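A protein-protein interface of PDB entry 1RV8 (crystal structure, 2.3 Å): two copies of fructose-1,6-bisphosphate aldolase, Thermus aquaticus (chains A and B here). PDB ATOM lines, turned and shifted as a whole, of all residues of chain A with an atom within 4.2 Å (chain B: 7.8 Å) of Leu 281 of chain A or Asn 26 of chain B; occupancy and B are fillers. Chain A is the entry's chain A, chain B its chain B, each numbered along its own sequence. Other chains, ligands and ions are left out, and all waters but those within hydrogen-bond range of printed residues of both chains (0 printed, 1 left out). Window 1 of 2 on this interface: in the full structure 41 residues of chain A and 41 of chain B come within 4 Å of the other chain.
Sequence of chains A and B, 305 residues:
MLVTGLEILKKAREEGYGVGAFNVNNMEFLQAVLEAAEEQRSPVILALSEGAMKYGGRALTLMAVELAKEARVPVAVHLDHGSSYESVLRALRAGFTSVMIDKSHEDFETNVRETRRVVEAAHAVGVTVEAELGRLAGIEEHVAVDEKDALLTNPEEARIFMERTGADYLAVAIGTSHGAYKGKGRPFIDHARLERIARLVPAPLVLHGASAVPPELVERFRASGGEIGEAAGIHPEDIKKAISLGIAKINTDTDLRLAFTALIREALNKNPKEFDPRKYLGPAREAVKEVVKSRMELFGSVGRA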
ATOM      1  N   MET A  27      21.883  16.701 -21.314  1.00  0.00           N
ATOM      2  CA  MET A  27      20.835  17.621 -20.898  1.00  0.00           C
ATOM      3  C   MET A  27      20.821  17.991 -19.420  1.00  0.00           C
ATOM      4  O   MET A  27      20.835  19.178 -19.080  1.00  0.00           O
ATOM      5  CB  MET A  27      19.458  17.072 -21.283  1.00  0.00           C
ATOM      6  CG  MET A  27      18.324  18.057 -21.063  1.00  0.00           C
ATOM      7  SD  MET A  27      16.700  17.295 -21.181  1.00  0.00           S
ATOM      8  CE  MET A  27      16.560  16.566 -19.514  1.00  0.00           C
ATOM      9  N   GLU A  28      20.800  17.012 -18.526  1.00  0.00           N
ATOM     10  CA  GLU A  28      20.743  17.398 -17.125  1.00  0.00           C
ATOM     11  C   GLU A  28      21.967  18.112 -16.554  1.00  0.00           C
ATOM     12  O   GLU A  28      21.819  18.927 -15.657  1.00  0.00           O
ATOM     13  CB  GLU A  28      20.304  16.231 -16.211  1.00  0.00           C
ATOM     14  CG  GLU A  28      20.637  14.822 -16.625  1.00  0.00           C
ATOM     15  CD  GLU A  28      19.819  14.315 -17.803  1.00  0.00           C
ATOM     16  OE1 GLU A  28      20.316  14.431 -18.937  1.00  0.00           O
ATOM     17  OE2 GLU A  28      18.693  13.799 -17.598  1.00  0.00           O
ATOM     18  N   ILE A 264      22.846   8.710  -8.433  1.00  0.00           N
ATOM     19  CA  ILE A 264      22.234   7.671  -9.247  1.00  0.00           C
ATOM     20  C   ILE A 264      22.353   6.339  -8.504  1.00  0.00           C
ATOM     21  O   ILE A 264      21.395   5.570  -8.429  1.00  0.00           O
ATOM     22  CB  ILE A 264      22.906   7.560 -10.638  1.00  0.00           C
ATOM     23  CG1 ILE A 264      22.598   8.819 -11.455  1.00  0.00           C
ATOM     24  CG2 ILE A 264      22.405   6.321 -11.368  1.00  0.00           C
ATOM     25  CD1 ILE A 264      23.053   8.749 -12.896  1.00  0.00           C
ATOM     26  N   PRO A 277      13.636   6.692 -15.527  1.00  0.00           N
ATOM     27  CA  PRO A 277      14.907   7.423 -15.438  1.00  0.00           C
ATOM     28  C   PRO A 277      14.881   8.797 -14.771  1.00  0.00           C
ATOM     29  O   PRO A 277      15.880   9.233 -14.206  1.00  0.00           O
ATOM     30  CB  PRO A 277      15.386   7.470 -16.892  1.00  0.00           C
ATOM     31  CG  PRO A 277      14.107   7.412 -17.678  1.00  0.00           C
ATOM     32  CD  PRO A 277      13.303   6.382 -16.927  1.00  0.00           C
ATOM     33  N   ARG A 278      13.748   9.478 -14.823  1.00  0.00           N
ATOM     34  CA  ARG A 278      13.649  10.793 -14.197  1.00  0.00           C
ATOM     35  C   ARG A 278      13.784  10.684 -12.683  1.00  0.00           C
ATOM     36  O   ARG A 278      14.265  11.605 -12.024  1.00  0.00           O
ATOM     37  CB  ARG A 278      12.312  11.446 -14.549  1.00  0.00           C
ATOM     38  CG  ARG A 278      12.172  11.726 -16.021  1.00  0.00           C
ATOM     39  CD  ARG A 278      10.726  11.966 -16.411  1.00  0.00           C
ATOM     40  NE  ARG A 278       9.877  10.828 -16.064  1.00  0.00           N
ATOM     41  CZ  ARG A 278       8.613  10.689 -16.456  1.00  0.00           C
ATOM     42  NH1 ARG A 278       8.043  11.614 -17.219  1.00  0.00           N
ATOM     43  NH2 ARG A 278       7.912   9.637 -16.065  1.00  0.00           N
ATOM     44  N   LYS A 279      13.366   9.545 -12.137  1.00  0.00           N
ATOM     45  CA  LYS A 279      13.421   9.322 -10.697  1.00  0.00           C
ATOM     46  C   LYS A 279      14.824   9.195 -10.118  1.00  0.00           C
ATOM     47  O   LYS A 279      15.036   9.496  -8.947  1.00  0.00           O
ATOM     48  CB  LYS A 279      12.585   8.098 -10.325  1.00  0.00           C
ATOM     49  CG  LYS A 279      11.086   8.304 -10.557  1.00  0.00           C
ATOM     50  CD  LYS A 279      10.532   9.384  -9.629  1.00  0.00           C
ATOM     51  CE  LYS A 279       9.129   9.812 -10.035  1.00  0.00           C
ATOM     52  NZ  LYS A 279       9.134  10.453 -11.384  1.00  0.00           N
ATOM     53  N   TYR A 280      15.787   8.741 -10.910  1.00  0.00           N
ATOM     54  CA  TYR A 280      17.138   8.653 -10.376  1.00  0.00           C
ATOM     55  C   TYR A 280      18.058   9.690 -11.017  1.00  0.00           C
ATOM     56  O   TYR A 280      19.040  10.111 -10.417  1.00  0.00           O
ATOM     57  CB  TYR A 280      17.703   7.226 -10.509  1.00  0.00           C
ATOM     58  CG  TYR A 280      17.558   6.569 -11.863  1.00  0.00           C
ATOM     59  CD1 TYR A 280      18.425   6.882 -12.913  1.00  0.00           C
ATOM     60  CD2 TYR A 280      16.575   5.601 -12.086  1.00  0.00           C
ATOM     61  CE1 TYR A 280      18.320   6.247 -14.144  1.00  0.00           C
ATOM     62  CE2 TYR A 280      16.461   4.959 -13.318  1.00  0.00           C
ATOM     63  CZ  TYR A 280      17.337   5.286 -14.340  1.00  0.00           C
ATOM     64  OH  TYR A 280      17.242   4.647 -15.549  1.00  0.00           O
ATOM     65  N   LEU A 281      17.720  10.124 -12.224  1.00  0.00           N
ATOM     66  CA  LEU A 281      18.512  11.129 -12.927  1.00  0.00           C
ATOM     67  C   LEU A 281      18.177  12.520 -12.378  1.00  0.00           C
ATOM     68  O   LEU A 281      19.029  13.410 -12.346  1.00  0.00           O
ATOM     69  CB  LEU A 281      18.206  11.068 -14.427  1.00  0.00           C
ATOM     70  CG  LEU A 281      19.183  10.401 -15.409  1.00  0.00           C
ATOM     71  CD1 LEU A 281      20.003   9.304 -14.741  1.00  0.00           C
ATOM     72  CD2 LEU A 281      18.379   9.862 -16.584  1.00  0.00           C
ATOM     73  N   GLY A 282      16.930  12.691 -11.943  1.00  0.00           N
ATOM     74  CA  GLY A 282      16.482  13.965 -11.405  1.00  0.00           C
ATOM     75  C   GLY A 282      17.247  14.413 -10.171  1.00  0.00           C
ATOM     76  O   GLY A 282      17.761  15.530 -10.136  1.00  0.00           O
ATOM     77  N   PRO A 283      17.328  13.571  -9.130  1.00  0.00           N
ATOM     78  CA  PRO A 283      18.057  13.947  -7.915  1.00  0.00           C
ATOM     79  C   PRO A 283      19.561  14.075  -8.155  1.00  0.00           C
ATOM     80  O   PRO A 283      20.252  14.807  -7.442  1.00  0.00           O
ATOM     81  CB  PRO A 283      17.715  12.818  -6.946  1.00  0.00           C
ATOM     82  CG  PRO A 283      16.339  12.425  -7.373  1.00  0.00           C
ATOM     83  CD  PRO A 283      16.490  12.385  -8.883  1.00  0.00           C
ATOM     84  N   ALA A 284      20.059  13.358  -9.162  1.00  0.00           N
ATOM     85  CA  ALA A 284      21.479  13.391  -9.503  1.00  0.00           C
ATOM     86  C   ALA A 284      21.780  14.720 -10.168  1.00  0.00           C
ATOM     87  O   ALA A 284      22.858  15.287 -10.001  1.00  0.00           O
ATOM     88  CB  ALA A 284      21.825  12.237 -10.449  1.00  0.00           C
ATOM     89  N   ARG A 285      20.807  15.204 -10.928  1.00  0.00           N
ATOM     90  CA  ARG A 285      20.919  16.471 -11.625  1.00  0.00           C
ATOM     91  C   ARG A 285      20.910  17.582 -10.567  1.00  0.00           C
ATOM     92  O   ARG A 285      21.718  18.510 -10.614  1.00  0.00           O
ATOM     93  CB  ARG A 285      19.737  16.615 -12.596  1.00  0.00           C
ATOM     94  CG  ARG A 285      19.553  17.990 -13.231  1.00  0.00           C
ATOM     95  CD  ARG A 285      18.078  18.368 -13.194  1.00  0.00           C
ATOM     96  NE  ARG A 285      17.401  18.096 -14.449  1.00  0.00           N
ATOM     97  CZ  ARG A 285      16.087  17.907 -14.574  1.00  0.00           C
ATOM     98  NH1 ARG A 285      15.287  17.944 -13.514  1.00  0.00           N
ATOM     99  NH2 ARG A 285      15.567  17.700 -15.779  1.00  0.00           N
ATOM    100  N   ASN B  23       8.229   7.736 -26.342  1.00  0.00           N
ATOM    101  CA  ASN B  23       8.374   8.747 -25.303  1.00  0.00           C
ATOM    102  C   ASN B  23       9.844   8.990 -25.000  1.00  0.00           C
ATOM    103  O   ASN B  23      10.620   8.043 -24.903  1.00  0.00           O
ATOM    104  CB  ASN B  23       7.662   8.313 -24.018  1.00  0.00           C
ATOM    105  CG  ASN B  23       6.157   8.387 -24.132  1.00  0.00           C
ATOM    106  OD1 ASN B  23       5.518   7.508 -24.705  1.00  0.00           O
ATOM    107  ND2 ASN B  23       5.581   9.451 -23.598  1.00  0.00           N
ATOM    108  N   VAL B  24      10.220  10.259 -24.874  1.00  0.00           N
ATOM    109  CA  VAL B  24      11.597  10.632 -24.552  1.00  0.00           C
ATOM    110  C   VAL B  24      11.554  11.646 -23.421  1.00  0.00           C
ATOM    111  O   VAL B  24      10.587  12.388 -23.290  1.00  0.00           O
ATOM    112  CB  VAL B  24      12.322  11.265 -25.761  1.00  0.00           C
ATOM    113  CG1 VAL B  24      12.336  10.297 -26.922  1.00  0.00           C
ATOM    114  CG2 VAL B  24      11.646  12.566 -26.158  1.00  0.00           C
ATOM    115  N   ASN B  25      12.596  11.677 -22.601  1.00  0.00           N
ATOM    116  CA  ASN B  25      12.642  12.604 -21.479  1.00  0.00           C
ATOM    117  C   ASN B  25      13.967  13.363 -21.408  1.00  0.00           C
ATOM    118  O   ASN B  25      14.076  14.348 -20.681  1.00  0.00           O
ATOM    119  CB  ASN B  25      12.380  11.857 -20.157  1.00  0.00           C
ATOM    120  CG  ASN B  25      10.898  11.563 -19.924  1.00  0.00           C
ATOM    121  OD1 ASN B  25      10.137  12.436 -19.475  1.00  0.00           O
ATOM    122  ND2 ASN B  25      10.475  10.333 -20.238  1.00  0.00           N
ATOM    123  N   ASN B  26      14.977  12.905 -22.144  1.00  0.00           N
ATOM    124  CA  ASN B  26      16.262  13.599 -22.161  1.00  0.00           C
ATOM    125  C   ASN B  26      17.013  13.424 -23.484  1.00  0.00           C
ATOM    126  O   ASN B  26      16.478  12.880 -24.452  1.00  0.00           O
ATOM    127  CB  ASN B  26      17.151  13.157 -20.996  1.00  0.00           C
ATOM    128  CG  ASN B  26      17.540  11.687 -21.075  1.00  0.00           C
ATOM    129  OD1 ASN B  26      17.391  11.042 -22.115  1.00  0.00           O
ATOM    130  ND2 ASN B  26      18.044  11.155 -19.973  1.00  0.00           N
ATOM    131  N   MET B  27      18.254  13.901 -23.509  1.00  0.00           N
ATOM    132  CA  MET B  27      19.088  13.839 -24.701  1.00  0.00           C
ATOM    133  C   MET B  27      19.334  12.429 -25.215  1.00  0.00           C
ATOM    134  O   MET B  27      19.082  12.143 -26.384  1.00  0.00           O
ATOM    135  CB  MET B  27      20.427  14.530 -24.437  1.00  0.00           C
ATOM    136  CG  MET B  27      21.324  14.610 -25.664  1.00  0.00           C
ATOM    137  SD  MET B  27      22.988  15.159 -25.254  1.00  0.00           S
ATOM    138  CE  MET B  27      23.748  13.572 -24.803  1.00  0.00           C
ATOM    139  N   GLU B  28      19.825  11.552 -24.343  1.00  0.00           N
ATOM    140  CA  GLU B  28      20.108  10.174 -24.724  1.00  0.00           C
ATOM    141  C   GLU B  28      18.915   9.463 -25.355  1.00  0.00           C
ATOM    142  O   GLU B  28      19.066   8.792 -26.378  1.00  0.00           O
ATOM    143  CB  GLU B  28      20.591   9.359 -23.512  1.00  0.00           C
ATOM    144  CG  GLU B  28      22.015   9.660 -23.047  1.00  0.00           C
ATOM    145  CD  GLU B  28      22.104  10.890 -22.158  1.00  0.00           C
ATOM    146  OE1 GLU B  28      23.216  11.175 -21.653  1.00  0.00           O
ATOM    147  OE2 GLU B  28      21.065  11.566 -21.958  1.00  0.00           O
ATOM    148  N   PHE B  29      17.737   9.595 -24.749  1.00  0.00           N
ATOM    149  CA  PHE B  29      16.546   8.931 -25.289  1.00  0.00           C
ATOM    150  C   PHE B  29      16.195   9.486 -26.662  1.00  0.00           C
ATOM    151  O   PHE B  29      15.855   8.734 -27.578  1.00  0.00           O
ATOM    152  CB  PHE B  29      15.333   9.100 -24.359  1.00  0.00           C
ATOM    153  CG  PHE B  29      15.228   8.048 -23.285  1.00  0.00           C
ATOM    154  CD1 PHE B  29      16.077   8.065 -22.187  1.00  0.00           C
ATOM    155  CD2 PHE B  29      14.277   7.034 -23.381  1.00  0.00           C
ATOM    156  CE1 PHE B  29      15.981   7.088 -21.198  1.00  0.00           C
ATOM    157  CE2 PHE B  29      14.175   6.050 -22.396  1.00  0.00           C
ATOM    158  CZ  PHE B  29      15.029   6.077 -21.303  1.00  0.00           C
ATOM    159  N   LEU B  30      16.275  10.800 -26.798  1.00  0.00           N
ATOM    160  CA  LEU B  30      15.960  11.453 -28.066  1.00  0.00           C
ATOM    161  C   LEU B  30      16.952  11.039 -29.164  1.00  0.00           C
ATOM    162  O   LEU B  30      16.551  10.769 -30.295  1.00  0.00           O
ATOM    163  CB  LEU B  30      15.959  12.970 -27.872  1.00  0.00           C
ATOM    164  CG  LEU B  30      15.298  13.871 -28.918  1.00  0.00           C
ATOM    165  CD1 LEU B  30      13.909  13.356 -29.265  1.00  0.00           C
ATOM    166  CD2 LEU B  30      15.199  15.288 -28.350  1.00  0.00           C
ATOM    167  N   GLN B  31      18.240  10.982 -28.830  1.00  0.00           N
ATOM    168  CA  GLN B  31      19.251  10.584 -29.804  1.00  0.00           C
ATOM    169  C   GLN B  31      19.006   9.136 -30.213  1.00  0.00           C
ATOM    170  O   GLN B  31      19.092   8.784 -31.388  1.00  0.00           O
ATOM    171  CB  GLN B  31      20.661  10.709 -29.210  1.00  0.00           C
ATOM    172  CG  GLN B  31      21.140  12.136 -28.959  1.00  0.00           C
ATOM    173  CD  GLN B  31      22.446  12.165 -28.196  1.00  0.00           C
ATOM    174  OE1 GLN B  31      22.579  11.526 -27.152  1.00  0.00           O
ATOM    175  NE2 GLN B  31      23.423  12.904 -28.712  1.00  0.00           N
ATOM    176  N   ALA B  32      18.693   8.298 -29.235  1.00  0.00           N
ATOM    177  CA  ALA B  32      18.443   6.896 -29.506  1.00  0.00           C
ATOM    178  C   ALA B  32      17.293   6.718 -30.502  1.00  0.00           C
ATOM    179  O   ALA B  32      17.419   5.977 -31.475  1.00  0.00           O
ATOM    180  CB  ALA B  32      18.131   6.168 -28.207  1.00  0.00           C
ATOM    181  N   LEU B  48       6.255  13.384 -26.019  1.00  0.00           N
ATOM    182  CA  LEU B  48       6.652  13.969 -24.760  1.00  0.00           C
ATOM    183  C   LEU B  48       5.415  14.110 -23.878  1.00  0.00           C
ATOM    184  O   LEU B  48       4.464  14.817 -24.222  1.00  0.00           O
ATOM    185  CB  LEU B  48       7.313  15.338 -24.982  1.00  0.00           C
ATOM    186  CG  LEU B  48       8.737  15.404 -25.569  1.00  0.00           C
ATOM    187  CD1 LEU B  48       8.740  15.044 -27.054  1.00  0.00           C
ATOM    188  CD2 LEU B  48       9.281  16.809 -25.391  1.00  0.00           C
ATOM    189  N   ALA B  52       7.496  14.738 -19.111  1.00  0.00           N
ATOM    190  CA  ALA B  52       8.654  15.067 -19.930  1.00  0.00           C
ATOM    191  C   ALA B  52       8.773  16.581 -20.079  1.00  0.00           C
ATOM    192  O   ALA B  52       9.861  17.130 -19.962  1.00  0.00           O
ATOM    193  CB  ALA B  52       8.538  14.408 -21.301  1.00  0.00           C
ATOM    194  N   TYR B  55      10.148  17.784 -16.708  1.00  0.00           N
ATOM    195  CA  TYR B  55      11.510  17.344 -16.492  1.00  0.00           C
ATOM    196  C   TYR B  55      12.487  17.868 -17.543  1.00  0.00           C
ATOM    197  O   TYR B  55      13.547  18.382 -17.210  1.00  0.00           O
ATOM    198  CB  TYR B  55      11.543  15.819 -16.486  1.00  0.00           C
ATOM    199  CG  TYR B  55      12.919  15.249 -16.290  1.00  0.00           C
ATOM    200  CD1 TYR B  55      13.459  15.120 -15.011  1.00  0.00           C
ATOM    201  CD2 TYR B  55      13.690  14.838 -17.382  1.00  0.00           C
ATOM    202  CE1 TYR B  55      14.732  14.592 -14.818  1.00  0.00           C
ATOM    203  CE2 TYR B  55      14.969  14.310 -17.199  1.00  0.00           C
ATOM    204  CZ  TYR B  55      15.478  14.189 -15.911  1.00  0.00           C
ATOM    205  OH  TYR B  55      16.726  13.645 -15.704  1.00  0.00           O
ATOM    206  N   GLY B  56      12.128  17.719 -18.813  1.00  0.00           N
ATOM    207  CA  GLY B  56      12.998  18.154 -19.891  1.00  0.00           C
ATOM    208  C   GLY B  56      12.938  19.644 -20.146  1.00  0.00           C
ATOM    209  O   GLY B  56      13.930  20.248 -20.565  1.00  0.00           O
ATOM    210  N   ALA B  59      14.909  22.631 -22.663  1.00  0.00           N
ATOM    211  CA  ALA B  59      16.004  21.875 -23.260  1.00  0.00           C
ATOM    212  C   ALA B  59      15.486  20.733 -24.140  1.00  0.00           C
ATOM    213  O   ALA B  59      15.916  20.567 -25.278  1.00  0.00           O
ATOM    214  CB  ALA B  59      16.929  21.325 -22.165  1.00  0.00           C
ATOM    215  N   LEU B  60      14.548  19.960 -23.611  1.00  0.00           N
ATOM    216  CA  LEU B  60      13.984  18.828 -24.336  1.00  0.00           C
ATOM    217  C   LEU B  60      13.205  19.283 -25.561  1.00  0.00           C
ATOM    218  O   LEU B  60      13.427  18.786 -26.667  1.00  0.00           O
ATOM    219  CB  LEU B  60      13.043  18.033 -23.435  1.00  0.00           C
ATOM    220  CG  LEU B  60      13.136  16.506 -23.341  1.00  0.00           C
ATOM    221  CD1 LEU B  60      11.744  15.977 -23.059  1.00  0.00           C
ATOM    222  CD2 LEU B  60      13.701  15.874 -24.611  1.00  0.00           C
ATOM    223  N   MET B  63      15.477  20.493 -28.313  1.00  0.00           N
ATOM    224  CA  MET B  63      16.070  19.362 -29.021  1.00  0.00           C
ATOM    225  C   MET B  63      15.062  18.618 -29.905  1.00  0.00           C
ATOM    226  O   MET B  63      15.320  18.383 -31.091  1.00  0.00           O
ATOM    227  CB  MET B  63      16.676  18.358 -28.030  1.00  0.00           C
ATOM    228  CG  MET B  63      17.995  18.776 -27.389  1.00  0.00           C
ATOM    229  SD  MET B  63      18.750  17.384 -26.501  1.00  0.00           S
ATOM    230  CE  MET B  63      17.572  17.227 -25.103  1.00  0.00           C
ATOM    231  N   ALA B  64      13.920  18.247 -29.329  1.00  0.00           N
ATOM    232  CA  ALA B  64      12.906  17.508 -30.074  1.00  0.00           C
ATOM    233  C   ALA B  64      12.518  18.197 -31.369  1.00  0.00           C
ATOM    234  O   ALA B  64      12.562  17.592 -32.439  1.00  0.00           O
ATOM    235  CB  ALA B  64      11.660  17.279 -29.209  1.00  0.00           C
ATOM    236  N   LEU B  67      16.029  18.979 -33.775  1.00  0.00           N
ATOM    237  CA  LEU B  67      16.656  17.784 -34.331  1.00  0.00           C
ATOM    238  C   LEU B  67      15.688  17.121 -35.314  1.00  0.00           C
ATOM    239  O   LEU B  67      16.110  16.460 -36.265  1.00  0.00           O
ATOM    240  CB  LEU B  67      17.056  16.813 -33.213  1.00  0.00           C
ATOM    241  CG  LEU B  67      18.100  17.371 -32.228  1.00  0.00           C
ATOM    242  CD1 LEU B  67      18.293  16.414 -31.062  1.00  0.00           C
ATOM    243  CD2 LEU B  67      19.419  17.611 -32.971  1.00  0.00           C
ATOM    244  N   PHE B 260      16.923   0.988 -20.754  1.00  0.00           N
ATOM    245  CA  PHE B 260      17.795   2.056 -20.278  1.00  0.00           C
ATOM    246  C   PHE B 260      18.244   1.798 -18.840  1.00  0.00           C
ATOM    247  O   PHE B 260      19.436   1.836 -18.532  1.00  0.00           O
ATOM    248  CB  PHE B 260      17.068   3.405 -20.356  1.00  0.00           C
ATOM    249  CG  PHE B 260      17.967   4.601 -20.161  1.00  0.00           C
ATOM    250  CD1 PHE B 260      18.837   5.009 -21.168  1.00  0.00           C
ATOM    251  CD2 PHE B 260      17.923   5.333 -18.982  1.00  0.00           C
ATOM    252  CE1 PHE B 260      19.649   6.138 -21.006  1.00  0.00           C
ATOM    253  CE2 PHE B 260      18.727   6.462 -18.803  1.00  0.00           C
ATOM    254  CZ  PHE B 260      19.592   6.867 -19.817  1.00  0.00           C
ATOM    255  N   ILE B 264      22.153   0.658 -17.096  1.00  0.00           N
ATOM    256  CA  ILE B 264      22.838   1.513 -16.149  1.00  0.00           C
ATOM    257  C   ILE B 264      23.229   0.614 -14.974  1.00  0.00           C
ATOM    258  O   ILE B 264      24.353   0.675 -14.478  1.00  0.00           O
ATOM    259  CB  ILE B 264      21.932   2.678 -15.676  1.00  0.00           C
ATOM    260  CG1 ILE B 264      21.640   3.609 -16.862  1.00  0.00           C
ATOM    261  CG2 ILE B 264      22.608   3.441 -14.541  1.00  0.00           C
ATOM    262  CD1 ILE B 264      20.767   4.809 -16.533  1.00  0.00           C
ATOM    263  N   TYR B 280      28.240   4.792 -18.469  1.00  0.00           N
ATOM    264  CA  TYR B 280      27.073   3.960 -18.203  1.00  0.00           C
ATOM    265  C   TYR B 280      25.812   4.438 -18.910  1.00  0.00           C
ATOM    266  O   TYR B 280      24.881   3.665 -19.100  1.00  0.00           O
ATOM    267  CB  TYR B 280      26.819   3.809 -16.693  1.00  0.00           C
ATOM    268  CG  TYR B 280      26.790   5.086 -15.887  1.00  0.00           C
ATOM    269  CD1 TYR B 280      25.637   5.865 -15.806  1.00  0.00           C
ATOM    270  CD2 TYR B 280      27.915   5.504 -15.184  1.00  0.00           C
ATOM    271  CE1 TYR B 280      25.607   7.024 -15.046  1.00  0.00           C
ATOM    272  CE2 TYR B 280      27.894   6.661 -14.420  1.00  0.00           C
ATOM    273  CZ  TYR B 280      26.741   7.416 -14.354  1.00  0.00           C
ATOM    274  OH  TYR B 280      26.731   8.564 -13.593  1.00  0.00           O
ATOM    275  N   LEU B 281      25.777   5.704 -19.310  1.00  0.00           N
ATOM    276  CA  LEU B 281      24.610   6.243 -20.010  1.00  0.00           C
ATOM    277  C   LEU B 281      24.682   5.914 -21.499  1.00  0.00           C
ATOM    278  O   LEU B 281      23.659   5.682 -22.141  1.00  0.00           O
ATOM    279  CB  LEU B 281      24.519   7.756 -19.810  1.00  0.00           C
ATOM    280  CG  LEU B 281      24.106   8.250 -18.417  1.00  0.00           C
ATOM    281  CD1 LEU B 281      24.118   9.776 -18.369  1.00  0.00           C
ATOM    282  CD2 LEU B 281      22.719   7.738 -18.087  1.00  0.00           C
ATOM    283  N   ARG B 285      21.934   4.179 -23.684  1.00  0.00           N
ATOM    284  CA  ARG B 285      21.340   4.855 -24.827  1.00  0.00           C
ATOM    285  C   ARG B 285      21.225   3.875 -26.010  1.00  0.00           C
ATOM    286  O   ARG B 285      20.198   3.832 -26.690  1.00  0.00           O
ATOM    287  CB  ARG B 285      22.199   6.071 -25.201  1.00  0.00           C
ATOM    288  CG  ARG B 285      21.848   6.726 -26.519  1.00  0.00           C
ATOM    289  CD  ARG B 285      23.126   7.157 -27.218  1.00  0.00           C
ATOM    290  NE  ARG B 285      23.570   8.480 -26.822  1.00  0.00           N
ATOM    291  CZ  ARG B 285      24.845   8.874 -26.788  1.00  0.00           C
ATOM    292  NH1 ARG B 285      25.824   8.036 -27.116  1.00  0.00           N
ATOM    293  NH2 ARG B 285      25.134  10.125 -26.446  1.00  0.00           N
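OE2 of Glu 28 of chain A is in hydrogen-bond range of OH of Tyr 55 of chain B (2.7 Å).
O of Tyr 55 of chain B is in hydrogen-bond range of NH2 of Arg 285 of chain A (2.6 Å).
The guanidinium group (NH1) of Arg 278 of chain A sits close to the side-chain amide oxygen (OD1) of Asn 25 of chain B, 3.2 Å away.
The side-chain amide oxygen (OD1) of Asn 26 of chain B sits at hydrogen-bond distance from the backbone NH (N) of Phe 29 of chain B.
OD1 of Asn 26 of chain B is in hydrogen-bond range of N of Glu 28 of chain B (3.3 Å).
Among the printed residues, merely in contact across the chains: Leu 281 of chain A with Tyr 55 of chain B (3.2 Å), Met 27 of chain A with Asn 25 of chain B (3.5 Å), Tyr 280 of chain A with Phe 260 of chain B (3.6 Å), Met 27 of chain A with Tyr 55 of chain B (3.6 Å), Arg 278 of chain A with Tyr 55 of chain B (3.6 Å), Glu 28 of chain A with Asn 26 of chain B (3.6 Å), Leu 281 of chain A with Asn 26 of chain B (3.6 Å), Tyr 280 of chain A with Ile 264 of chain B (3.7 Å), Arg 278 of chain A with Ala 52 of chain B (3.7 Å), Met 27 of chain A with Ala 59 of chain B (3.7 Å), Ile 264 of chain A with Tyr 280 of chain B (3.7 Å), Met 27 of chain A with Asn 26 of chain B (3.8 Å), Gly 282 of chain A with Tyr 55 of chain B (3.9 Å), Met 27 of chain A with Gly 56 of chain B (3.9 Å), Pro 277 of chain A with Phe 260 of chain B (3.9 Å) and Pro 277 of chain A with Phe 29 of chain B (3.97 Å).
Of chain B, only Asn 26 (3.6 Å) and Tyr 55 (3.2 Å) come within 4 Å of Leu 281 of chain A.
Asn 26 of chain B touches just these residues of chain A: Met 27, Glu 28 and Leu 281.
Of the printed residues of chain B, Glu 28 of chain A touches Asn 26 and Tyr 55.
Of the printed residues of chain A, Ile 264 of chain B touches Tyr 280.
The nearest residue of chain B that does not touch Leu 281 of chain A is Phe 260 of chain B (4.1 Å).
Of the 24 printed residues of chain B, 10 touch a printed residue of chain A.
Hydrophobic or aromatic side chains of chain B within 4 Å of the printed part of chain A: Phe 29, Tyr 55, Ala 59, Phe 260, Ile 264 and Tyr 280.
Ile 264 of chain A touches Tyr 280 of chain B, and with the chains exchanged Tyr 280 of chain A touches Ile 264 of chain B.
Of the 19 pairs that touch across the chains among the printed residues, 2 have their exchanged pair printed and touching as well.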
